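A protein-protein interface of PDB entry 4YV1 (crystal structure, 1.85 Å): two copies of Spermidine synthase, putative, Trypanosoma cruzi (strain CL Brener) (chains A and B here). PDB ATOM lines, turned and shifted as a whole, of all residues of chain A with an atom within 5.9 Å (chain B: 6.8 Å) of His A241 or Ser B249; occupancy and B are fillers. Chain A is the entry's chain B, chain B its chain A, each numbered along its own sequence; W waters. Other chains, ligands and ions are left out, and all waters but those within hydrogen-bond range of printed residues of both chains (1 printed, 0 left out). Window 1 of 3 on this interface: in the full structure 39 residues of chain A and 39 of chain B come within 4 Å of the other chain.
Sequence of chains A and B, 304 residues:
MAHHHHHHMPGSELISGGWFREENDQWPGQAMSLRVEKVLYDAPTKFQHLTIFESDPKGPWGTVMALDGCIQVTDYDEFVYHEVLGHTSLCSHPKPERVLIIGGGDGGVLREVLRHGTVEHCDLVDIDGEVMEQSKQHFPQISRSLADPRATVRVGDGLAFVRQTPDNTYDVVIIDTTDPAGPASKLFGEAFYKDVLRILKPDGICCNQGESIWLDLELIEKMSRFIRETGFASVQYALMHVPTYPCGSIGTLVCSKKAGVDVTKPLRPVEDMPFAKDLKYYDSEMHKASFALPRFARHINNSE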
ATOM      1  N   VAL A  80      23.658  25.974  16.826  1.00  0.00           N
ATOM      2  CA  VAL A  80      22.799  24.966  16.112  1.00  0.00           C
ATOM      3  C   VAL A  80      23.557  23.672  15.859  1.00  0.00           C
ATOM      4  O   VAL A  80      23.190  22.637  16.409  1.00  0.00           O
ATOM      5  CB  VAL A  80      22.257  25.438  14.725  1.00  0.00           C
ATOM      6  CG1 VAL A  80      21.294  24.349  14.162  1.00  0.00           C
ATOM      7  CG2 VAL A  80      21.494  26.770  14.910  1.00  0.00           C
ATOM      8  N   LEU A 239      18.206  16.631   9.975  1.00  0.00           N
ATOM      9  CA  LEU A 239      18.255  17.931   9.295  1.00  0.00           C
ATOM     10  C   LEU A 239      18.202  19.084  10.305  1.00  0.00           C
ATOM     11  O   LEU A 239      17.442  19.052  11.262  1.00  0.00           O
ATOM     12  CB  LEU A 239      16.999  18.057   8.348  1.00  0.00           C
ATOM     13  CG  LEU A 239      16.856  19.223   7.417  1.00  0.00           C
ATOM     14  CD1 LEU A 239      18.013  19.475   6.446  1.00  0.00           C
ATOM     15  CD2 LEU A 239      15.561  18.950   6.609  1.00  0.00           C
ATOM     16  N   MET A 240      18.949  20.150  10.052  1.00  0.00           N
ATOM     17  CA  MET A 240      18.907  21.289  10.960  1.00  0.00           C
ATOM     18  C   MET A 240      19.087  22.594  10.181  1.00  0.00           C
ATOM     19  O   MET A 240      19.594  22.623   9.057  1.00  0.00           O
ATOM     20  CB  MET A 240      20.054  21.154  12.040  1.00  0.00           C
ATOM     21  CG  MET A 240      21.451  21.418  11.425  1.00  0.00           C
ATOM     22  SD  MET A 240      22.834  20.774  12.482  1.00  0.00           S
ATOM     23  CE  MET A 240      23.091  19.107  11.819  1.00  0.00           C
ATOM     24  N   HIS A 241      18.685  23.681  10.808  1.00  0.00           N
ATOM     25  CA  HIS A 241      18.632  25.001  10.174  1.00  0.00           C
ATOM     26  C   HIS A 241      19.889  25.791  10.528  1.00  0.00           C
ATOM     27  O   HIS A 241      20.056  26.182  11.687  1.00  0.00           O
ATOM     28  CB  HIS A 241      17.460  25.751  10.821  1.00  0.00           C
ATOM     29  CG  HIS A 241      16.131  25.337  10.308  1.00  0.00           C
ATOM     30  ND1 HIS A 241      15.386  24.323  10.883  1.00  0.00           N
ATOM     31  CD2 HIS A 241      15.392  25.814   9.290  1.00  0.00           C
ATOM     32  CE1 HIS A 241      14.262  24.172  10.205  1.00  0.00           C
ATOM     33  NE2 HIS A 241      14.258  25.037   9.224  1.00  0.00           N
ATOM     34  N   VAL A 242      20.759  26.029   9.549  1.00  0.00           N
ATOM     35  CA  VAL A 242      21.964  26.794   9.802  1.00  0.00           C
ATOM     36  C   VAL A 242      22.052  27.873   8.740  1.00  0.00           C
ATOM     37  O   VAL A 242      22.448  27.590   7.580  1.00  0.00           O
ATOM     38  CB  VAL A 242      23.255  25.933   9.766  1.00  0.00           C
ATOM     39  CG1 VAL A 242      24.455  26.817  10.103  1.00  0.00           C
ATOM     40  CG2 VAL A 242      23.167  24.758  10.769  1.00  0.00           C
ATOM     41  N   PRO A 243      21.770  29.117   9.137  1.00  0.00           N
ATOM     42  CA  PRO A 243      21.659  30.123   8.075  1.00  0.00           C
ATOM     43  C   PRO A 243      22.951  30.445   7.327  1.00  0.00           C
ATOM     44  O   PRO A 243      22.905  30.964   6.187  1.00  0.00           O
ATOM     45  CB  PRO A 243      21.221  31.397   8.818  1.00  0.00           C
ATOM     46  CG  PRO A 243      20.898  31.006  10.210  1.00  0.00           C
ATOM     47  CD  PRO A 243      21.462  29.627  10.487  1.00  0.00           C
ATOM     48  N   GLY A 248      21.252  27.124   3.542  1.00  0.00           N
ATOM     49  CA  GLY A 248      20.586  27.360   4.847  1.00  0.00           C
ATOM     50  C   GLY A 248      20.307  26.159   5.728  1.00  0.00           C
ATOM     51  O   GLY A 248      19.601  26.273   6.757  1.00  0.00           O
ATOM     52  N   SER A 249      20.877  25.018   5.356  1.00  0.00           N
ATOM     53  CA  SER A 249      20.714  23.792   6.169  1.00  0.00           C
ATOM     54  C   SER A 249      21.893  22.826   6.006  1.00  0.00           C
ATOM     55  O   SER A 249      22.719  22.981   5.101  1.00  0.00           O
ATOM     56  CB  SER A 249      19.410  23.075   5.878  1.00  0.00           C
ATOM     57  OG  SER A 249      19.388  22.539   4.581  1.00  0.00           O
ATOM     58  N   ILE A 250      21.969  21.872   6.923  1.00  0.00           N
ATOM     59  CA  ILE A 250      22.955  20.826   6.868  1.00  0.00           C
ATOM     60  C   ILE A 250      22.365  19.669   7.691  1.00  0.00           C
ATOM     61  O   ILE A 250      21.313  19.805   8.366  1.00  0.00           O
ATOM     62  CB  ILE A 250      24.310  21.350   7.430  1.00  0.00           C
ATOM     63  CG1 ILE A 250      25.403  20.458   6.885  1.00  0.00           C
ATOM     64  CG2 ILE A 250      24.308  21.409   8.956  1.00  0.00           C
ATOM     65  CD1 ILE A 250      26.836  20.938   7.173  1.00  0.00           C
ATOM     66  N   TYR A 281      19.010  25.780  20.842  1.00  0.00           N
ATOM     67  CA  TYR A 281      18.334  25.165  19.686  1.00  0.00           C
ATOM     68  C   TYR A 281      17.651  23.847  20.057  1.00  0.00           C
ATOM     69  O   TYR A 281      16.430  23.678  19.913  1.00  0.00           O
ATOM     70  CB  TYR A 281      19.353  24.986  18.581  1.00  0.00           C
ATOM     71  CG  TYR A 281      18.759  24.410  17.247  1.00  0.00           C
ATOM     72  CD1 TYR A 281      18.668  23.024  17.048  1.00  0.00           C
ATOM     73  CD2 TYR A 281      18.360  25.283  16.205  1.00  0.00           C
ATOM     74  CE1 TYR A 281      18.150  22.499  15.852  1.00  0.00           C
ATOM     75  CE2 TYR A 281      17.863  24.790  14.986  1.00  0.00           C
ATOM     76  CZ  TYR A 281      17.769  23.420  14.813  1.00  0.00           C
ATOM     77  OH  TYR A 281      17.275  22.913  13.628  1.00  0.00           O
ATOM     78  N   MET A 286      12.717  19.169  18.964  1.00  0.00           N
ATOM     79  CA  MET A 286      13.579  19.388  17.805  1.00  0.00           C
ATOM     80  C   MET A 286      14.295  18.118  17.364  1.00  0.00           C
ATOM     81  O   MET A 286      14.481  17.887  16.155  1.00  0.00           O
ATOM     82  CB  MET A 286      14.600  20.509  17.985  1.00  0.00           C
ATOM     83  CG  MET A 286      13.967  21.889  18.171  1.00  0.00           C
ATOM     84  SD  MET A 286      13.175  22.336  16.600  1.00  0.00           S
ATOM     85  CE  MET A 286      14.471  22.637  15.473  1.00  0.00           C
ATOM     86  N   GLU B 211       7.594  35.290   7.821  1.00  0.00           N
ATOM     87  CA  GLU B 211       8.847  35.971   8.199  1.00  0.00           C
ATOM     88  C   GLU B 211       9.863  35.003   8.826  1.00  0.00           C
ATOM     89  O   GLU B 211       9.525  33.828   9.101  1.00  0.00           O
ATOM     90  CB  GLU B 211       8.544  37.098   9.206  1.00  0.00           C
ATOM     91  CG  GLU B 211       7.613  38.162   8.662  1.00  0.00           C
ATOM     92  CD  GLU B 211       8.270  38.863   7.506  1.00  0.00           C
ATOM     93  OE1 GLU B 211       9.270  39.557   7.762  1.00  0.00           O
ATOM     94  OE2 GLU B 211       7.826  38.681   6.346  1.00  0.00           O
ATOM     95  N   SER B 212      11.075  35.497   9.060  1.00  0.00           N
ATOM     96  CA  SER B 212      12.210  34.620   9.421  1.00  0.00           C
ATOM     97  C   SER B 212      12.522  34.669  10.944  1.00  0.00           C
ATOM     98  O   SER B 212      12.557  35.768  11.550  1.00  0.00           O
ATOM     99  CB  SER B 212      13.419  35.081   8.637  1.00  0.00           C
ATOM    100  OG  SER B 212      14.634  34.649   9.228  1.00  0.00           O
ATOM    101  N   ILE B 213      12.746  33.507  11.584  1.00  0.00           N
ATOM    102  CA  ILE B 213      13.107  33.494  13.013  1.00  0.00           C
ATOM    103  C   ILE B 213      14.521  34.016  13.297  1.00  0.00           C
ATOM    104  O   ILE B 213      14.849  34.336  14.478  1.00  0.00           O
ATOM    105  CB  ILE B 213      12.979  32.058  13.602  1.00  0.00           C
ATOM    106  CG1 ILE B 213      14.013  31.070  12.949  1.00  0.00           C
ATOM    107  CG2 ILE B 213      11.537  31.630  13.528  1.00  0.00           C
ATOM    108  CD1 ILE B 213      13.989  29.716  13.704  1.00  0.00           C
ATOM    109  N   TRP B 214      15.370  34.063  12.253  1.00  0.00           N
ATOM    110  CA  TRP B 214      16.734  34.613  12.320  1.00  0.00           C
ATOM    111  C   TRP B 214      16.804  36.149  12.224  1.00  0.00           C
ATOM    112  O   TRP B 214      17.653  36.786  12.859  1.00  0.00           O
ATOM    113  CB  TRP B 214      17.624  33.981  11.260  1.00  0.00           C
ATOM    114  CG  TRP B 214      17.746  32.526  11.472  1.00  0.00           C
ATOM    115  CD1 TRP B 214      17.114  31.561  10.760  1.00  0.00           C
ATOM    116  CD2 TRP B 214      18.494  31.863  12.497  1.00  0.00           C
ATOM    117  NE1 TRP B 214      17.417  30.323  11.276  1.00  0.00           N
ATOM    118  CE2 TRP B 214      18.307  30.479  12.316  1.00  0.00           C
ATOM    119  CE3 TRP B 214      19.365  32.313  13.528  1.00  0.00           C
ATOM    120  CZ2 TRP B 214      18.956  29.486  13.153  1.00  0.00           C
ATOM    121  CZ3 TRP B 214      20.032  31.320  14.380  1.00  0.00           C
ATOM    122  CH2 TRP B 214      19.808  29.928  14.158  1.00  0.00           C
ATOM    123  N   TYR B 237       3.269  28.976  14.683  1.00  0.00           N
ATOM    124  CA  TYR B 237       4.154  29.267  13.535  1.00  0.00           C
ATOM    125  C   TYR B 237       4.751  27.951  13.035  1.00  0.00           C
ATOM    126  O   TYR B 237       5.256  27.087  13.844  1.00  0.00           O
ATOM    127  CB  TYR B 237       5.241  30.279  14.032  1.00  0.00           C
ATOM    128  CG  TYR B 237       6.365  30.615  13.085  1.00  0.00           C
ATOM    129  CD1 TYR B 237       7.488  29.761  12.970  1.00  0.00           C
ATOM    130  CD2 TYR B 237       6.351  31.803  12.383  1.00  0.00           C
ATOM    131  CE1 TYR B 237       8.530  30.057  12.141  1.00  0.00           C
ATOM    132  CE2 TYR B 237       7.403  32.140  11.548  1.00  0.00           C
ATOM    133  CZ  TYR B 237       8.499  31.270  11.462  1.00  0.00           C
ATOM    134  OH  TYR B 237       9.560  31.563  10.649  1.00  0.00           O
ATOM    135  N   LEU B 239       7.561  26.339  10.600  1.00  0.00           N
ATOM    136  CA  LEU B 239       8.828  26.740  10.012  1.00  0.00           C
ATOM    137  C   LEU B 239       9.119  25.843   8.770  1.00  0.00           C
ATOM    138  O   LEU B 239       8.797  24.651   8.792  1.00  0.00           O
ATOM    139  CB  LEU B 239       9.914  26.480  11.146  1.00  0.00           C
ATOM    140  CG  LEU B 239      11.392  26.690  10.860  1.00  0.00           C
ATOM    141  CD1 LEU B 239      11.743  28.141  10.507  1.00  0.00           C
ATOM    142  CD2 LEU B 239      12.182  26.212  12.105  1.00  0.00           C
ATOM    143  N   MET B 240       9.750  26.392   7.735  1.00  0.00           N
ATOM    144  CA  MET B 240      10.069  25.558   6.556  1.00  0.00           C
ATOM    145  C   MET B 240      11.448  25.938   6.000  1.00  0.00           C
ATOM    146  O   MET B 240      11.929  27.044   6.194  1.00  0.00           O
ATOM    147  CB  MET B 240       8.995  25.694   5.454  1.00  0.00           C
ATOM    148  CG  MET B 240       8.975  27.105   4.861  1.00  0.00           C
ATOM    149  SD  MET B 240       7.407  27.479   3.994  1.00  0.00           S
ATOM    150  CE  MET B 240       6.445  28.357   5.265  1.00  0.00           C
ATOM    151  N   HIS B 241      12.049  25.006   5.265  1.00  0.00           N
ATOM    152  CA  HIS B 241      13.358  25.227   4.632  1.00  0.00           C
ATOM    153  C   HIS B 241      13.251  25.784   3.198  1.00  0.00           C
ATOM    154  O   HIS B 241      12.823  25.068   2.319  1.00  0.00           O
ATOM    155  CB  HIS B 241      13.987  23.854   4.555  1.00  0.00           C
ATOM    156  CG  HIS B 241      14.430  23.312   5.870  1.00  0.00           C
ATOM    157  ND1 HIS B 241      13.677  22.437   6.635  1.00  0.00           N
ATOM    158  CD2 HIS B 241      15.616  23.440   6.506  1.00  0.00           C
ATOM    159  CE1 HIS B 241      14.359  22.121   7.728  1.00  0.00           C
ATOM    160  NE2 HIS B 241      15.545  22.694   7.653  1.00  0.00           N
ATOM    161  N   VAL B 242      13.693  27.031   2.947  1.00  0.00           N
ATOM    162  CA  VAL B 242      13.615  27.633   1.616  1.00  0.00           C
ATOM    163  C   VAL B 242      14.976  28.255   1.321  1.00  0.00           C
ATOM    164  O   VAL B 242      15.360  29.323   1.861  1.00  0.00           O
ATOM    165  CB  VAL B 242      12.506  28.695   1.470  1.00  0.00           C
ATOM    166  CG1 VAL B 242      12.430  29.209   0.049  1.00  0.00           C
ATOM    167  CG2 VAL B 242      11.117  28.127   1.824  1.00  0.00           C
ATOM    168  N   PRO B 243      15.722  27.570   0.461  1.00  0.00           N
ATOM    169  CA  PRO B 243      17.140  27.911   0.245  1.00  0.00           C
ATOM    170  C   PRO B 243      17.314  29.343  -0.274  1.00  0.00           C
ATOM    171  O   PRO B 243      18.276  30.064   0.110  1.00  0.00           O
ATOM    172  CB  PRO B 243      17.594  26.876  -0.786  1.00  0.00           C
ATOM    173  CG  PRO B 243      16.610  25.767  -0.740  1.00  0.00           C
ATOM    174  CD  PRO B 243      15.318  26.319  -0.215  1.00  0.00           C
ATOM    175  N   THR B 244      16.330  29.839  -1.019  1.00  0.00           N
ATOM    176  CA  THR B 244      16.561  31.164  -1.642  1.00  0.00           C
ATOM    177  C   THR B 244      15.971  32.297  -0.818  1.00  0.00           C
ATOM    178  O   THR B 244      15.915  33.437  -1.285  1.00  0.00           O
ATOM    179  CB  THR B 244      15.894  31.211  -3.033  1.00  0.00           C
ATOM    180  OG1 THR B 244      14.551  30.743  -2.875  1.00  0.00           O
ATOM    181  CG2 THR B 244      16.612  30.311  -4.055  1.00  0.00           C
ATOM    182  N   TYR B 245      15.444  32.012   0.368  1.00  0.00           N
ATOM    183  CA  TYR B 245      14.962  33.119   1.176  1.00  0.00           C
ATOM    184  C   TYR B 245      16.061  33.473   2.160  1.00  0.00           C
ATOM    185  O   TYR B 245      16.901  32.613   2.491  1.00  0.00           O
ATOM    186  CB  TYR B 245      13.610  32.783   1.861  1.00  0.00           C
ATOM    187  CG  TYR B 245      12.365  32.784   0.916  1.00  0.00           C
ATOM    188  CD1 TYR B 245      12.362  33.436  -0.338  1.00  0.00           C
ATOM    189  CD2 TYR B 245      11.168  32.166   1.313  1.00  0.00           C
ATOM    190  CE1 TYR B 245      11.215  33.428  -1.168  1.00  0.00           C
ATOM    191  CE2 TYR B 245      10.026  32.165   0.493  1.00  0.00           C
ATOM    192  CZ  TYR B 245      10.039  32.812  -0.741  1.00  0.00           C
ATOM    193  OH  TYR B 245       8.869  32.798  -1.513  1.00  0.00           O
ATOM    194  N   PRO B 246      16.088  34.743   2.624  1.00  0.00           N
ATOM    195  CA  PRO B 246      17.117  35.223   3.543  1.00  0.00           C
ATOM    196  C   PRO B 246      17.303  34.255   4.764  1.00  0.00           C
ATOM    197  O   PRO B 246      16.310  33.915   5.435  1.00  0.00           O
ATOM    198  CB  PRO B 246      16.495  36.505   4.079  1.00  0.00           C
ATOM    199  CG  PRO B 246      15.612  37.028   2.959  1.00  0.00           C
ATOM    200  CD  PRO B 246      15.075  35.799   2.299  1.00  0.00           C
ATOM    201  N   CYS B 247      18.548  33.849   5.009  1.00  0.00           N
ATOM    202  CA  CYS B 247      18.946  32.880   6.040  1.00  0.00           C
ATOM    203  C   CYS B 247      18.363  31.475   5.886  1.00  0.00           C
ATOM    204  O   CYS B 247      18.402  30.711   6.854  1.00  0.00           O
ATOM    205  CB  CYS B 247      18.637  33.418   7.457  1.00  0.00           C
ATOM    206  SG  CYS B 247      19.725  34.790   7.941  1.00  0.00           S
ATOM    207  N   GLY B 248      17.781  31.180   4.739  1.00  0.00           N
ATOM    208  CA  GLY B 248      17.338  29.808   4.356  1.00  0.00           C
ATOM    209  C   GLY B 248      16.071  29.182   4.924  1.00  0.00           C
ATOM    210  O   GLY B 248      15.818  27.977   4.769  1.00  0.00           O
ATOM    211  N   SER B 249      15.241  30.003   5.550  1.00  0.00           N
ATOM    212  CA  SER B 249      13.973  29.526   6.101  1.00  0.00           C
ATOM    213  C   SER B 249      12.974  30.697   6.098  1.00  0.00           C
ATOM    214  O   SER B 249      13.342  31.896   5.836  1.00  0.00           O
ATOM    215  CB  SER B 249      14.127  28.920   7.484  1.00  0.00           C
ATOM    216  OG  SER B 249      14.519  29.928   8.417  1.00  0.00           O
ATOM    217  N   ILE B 250      11.706  30.323   6.234  1.00  0.00           N
ATOM    218  CA  ILE B 250      10.648  31.272   6.398  1.00  0.00           C
ATOM    219  C   ILE B 250       9.588  30.514   7.139  1.00  0.00           C
ATOM    220  O   ILE B 250       9.761  29.333   7.429  1.00  0.00           O
ATOM    221  CB  ILE B 250      10.158  31.879   5.071  1.00  0.00           C
ATOM    222  CG1 ILE B 250       9.505  33.240   5.360  1.00  0.00           C
ATOM    223  CG2 ILE B 250       9.262  30.881   4.336  1.00  0.00           C
ATOM    224  CD1 ILE B 250       9.064  34.018   4.128  1.00  0.00           C
ATOM    225  N   GLY B 251       8.522  31.195   7.589  1.00  0.00           N
ATOM    226  CA  GLY B 251       7.479  30.435   8.263  1.00  0.00           C
ATOM    227  C   GLY B 251       6.080  30.951   7.857  1.00  0.00           C
ATOM    228  O   GLY B 251       5.944  31.848   7.014  1.00  0.00           O
ATOM    229  N   TYR B 281       7.574  18.251  -1.008  1.00  0.00           N
ATOM    230  CA  TYR B 281       8.066  18.647   0.323  1.00  0.00           C
ATOM    231  C   TYR B 281       7.121  18.118   1.400  1.00  0.00           C
ATOM    232  O   TYR B 281       7.554  17.349   2.258  1.00  0.00           O
ATOM    233  CB  TYR B 281       8.180  20.175   0.399  1.00  0.00           C
ATOM    234  CG  TYR B 281       8.741  20.754   1.707  1.00  0.00           C
ATOM    235  CD1 TYR B 281       7.910  21.024   2.800  1.00  0.00           C
ATOM    236  CD2 TYR B 281      10.128  20.987   1.833  1.00  0.00           C
ATOM    237  CE1 TYR B 281       8.434  21.565   3.989  1.00  0.00           C
ATOM    238  CE2 TYR B 281      10.683  21.558   2.983  1.00  0.00           C
ATOM    239  CZ  TYR B 281       9.837  21.829   4.061  1.00  0.00           C
ATOM    240  OH  TYR B 281      10.415  22.414   5.179  1.00  0.00           O
ATOM    241  N   ALA B 292       7.726  22.352  15.402  1.00  0.00           N
ATOM    242  CA  ALA B 292       8.803  22.244  16.403  1.00  0.00           C
ATOM    243  C   ALA B 292       9.810  23.368  16.143  1.00  0.00           C
ATOM    244  O   ALA B 292      10.496  23.409  15.092  1.00  0.00           O
ATOM    245  CB  ALA B 292       9.433  20.870  16.319  1.00  0.00           C
ATOM    246  N   PRO B 294      13.176  25.896  17.253  1.00  0.00           N
ATOM    247  CA  PRO B 294      14.408  25.950  18.079  1.00  0.00           C
ATOM    248  C   PRO B 294      14.068  26.581  19.441  1.00  0.00           C
ATOM    249  O   PRO B 294      13.207  27.456  19.518  1.00  0.00           O
ATOM    250  CB  PRO B 294      15.278  26.921  17.295  1.00  0.00           C
ATOM    251  CG  PRO B 294      14.893  26.609  15.852  1.00  0.00           C
ATOM    252  CD  PRO B 294      13.398  26.457  15.907  1.00  0.00           C
HETATM  253  O   HOH W   1      14.586  20.331   9.940  1.00  0.00           O
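NE2 of His A241 sits at hydrogen-bond distance from NE2 of His B241 (3.1 Å). The backbone carbonyl oxygen (O) of Ala B292 lies close to the side-chain sulfur (SD) of Met A286 (3.3 Å). The side-chain sulfur (SD) of Met A286 sits close to the backbone nitrogen (N) of Pro B294 (3.6 Å).
The backbone NH (N) of Trp B214 is in hydrogen-bond range of the side-chain hydroxyl (OG) of Ser B212, 3.2 Å away. The side-chain hydroxyl of Tyr B281 sits at hydrogen-bond distance from the backbone NH of His B241. N of His A241 is in hydrogen-bond range of OH of Tyr A281 (3.2 Å).
Among the printed residues, merely in contact across the chains: Val A80 with Trp B214 (3.7 Å), Leu A239 with His B241 (3.6 Å), His A241 with Trp B214 (3.8 Å), His A241 with Leu B239 (3.5 Å), His A241 with Ser B249 (3.8 Å), Pro A243 with Trp B214 (3.4 Å), Pro A243 with Cys B247 (3.5 Å), Ser A249 with His B241 (3.9 Å) and Tyr A281 with Pro B294 (3.6 Å).
Of chain B, only Trp B214, Leu B239, His B241 and Ser B249 come within 4 Å of His A241. Of chain A, only His A241 comes within 4 Å of Ser B249. Printed residues of chain A within 4 Å of Cys B247: Pro A243 (3.5 Å). Of the printed residues of chain B, Pro A243 touches Trp B214 and Cys B247. Of the printed residues of chain B, Leu A239 touches His B241 (3.6 Å). Of the printed residues of chain B, Tyr A281 touches Pro B294. Met A240 touches none of the printed residues of chain B. The nearest printed residue of chain B that does not touch Tyr A281 is Trp B214 (5.2 Å).
Of the 11 printed residues of chain A, 7 touch a printed residue of chain B. Of the 21 printed residues of chain B, 7 touch a printed residue of chain A. Hydrophobic or aromatic side chains of chain B within 4 Å of the printed part of chain A: Trp B214, Leu B239, His B241 and Pro B294. Among the printed residues, no Asp or Glu carboxylate lies within 4 Å of a Lys or Arg side-chain nitrogen of the other chain.
Leu A239 touches His B241, and with the chains exchanged His A241 touches Leu B239. His B241 touches its own counterpart, His A241. His A241 touches Ser B249, and with the chains exchanged Ser A249 touches His B241. 9 positions are printed for both chains.
Water W1 bridges the backbone carbonyl oxygen of Leu A239 (3.4 Å) and a ring nitrogen (NE2) of His B241 (3.4 Å).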
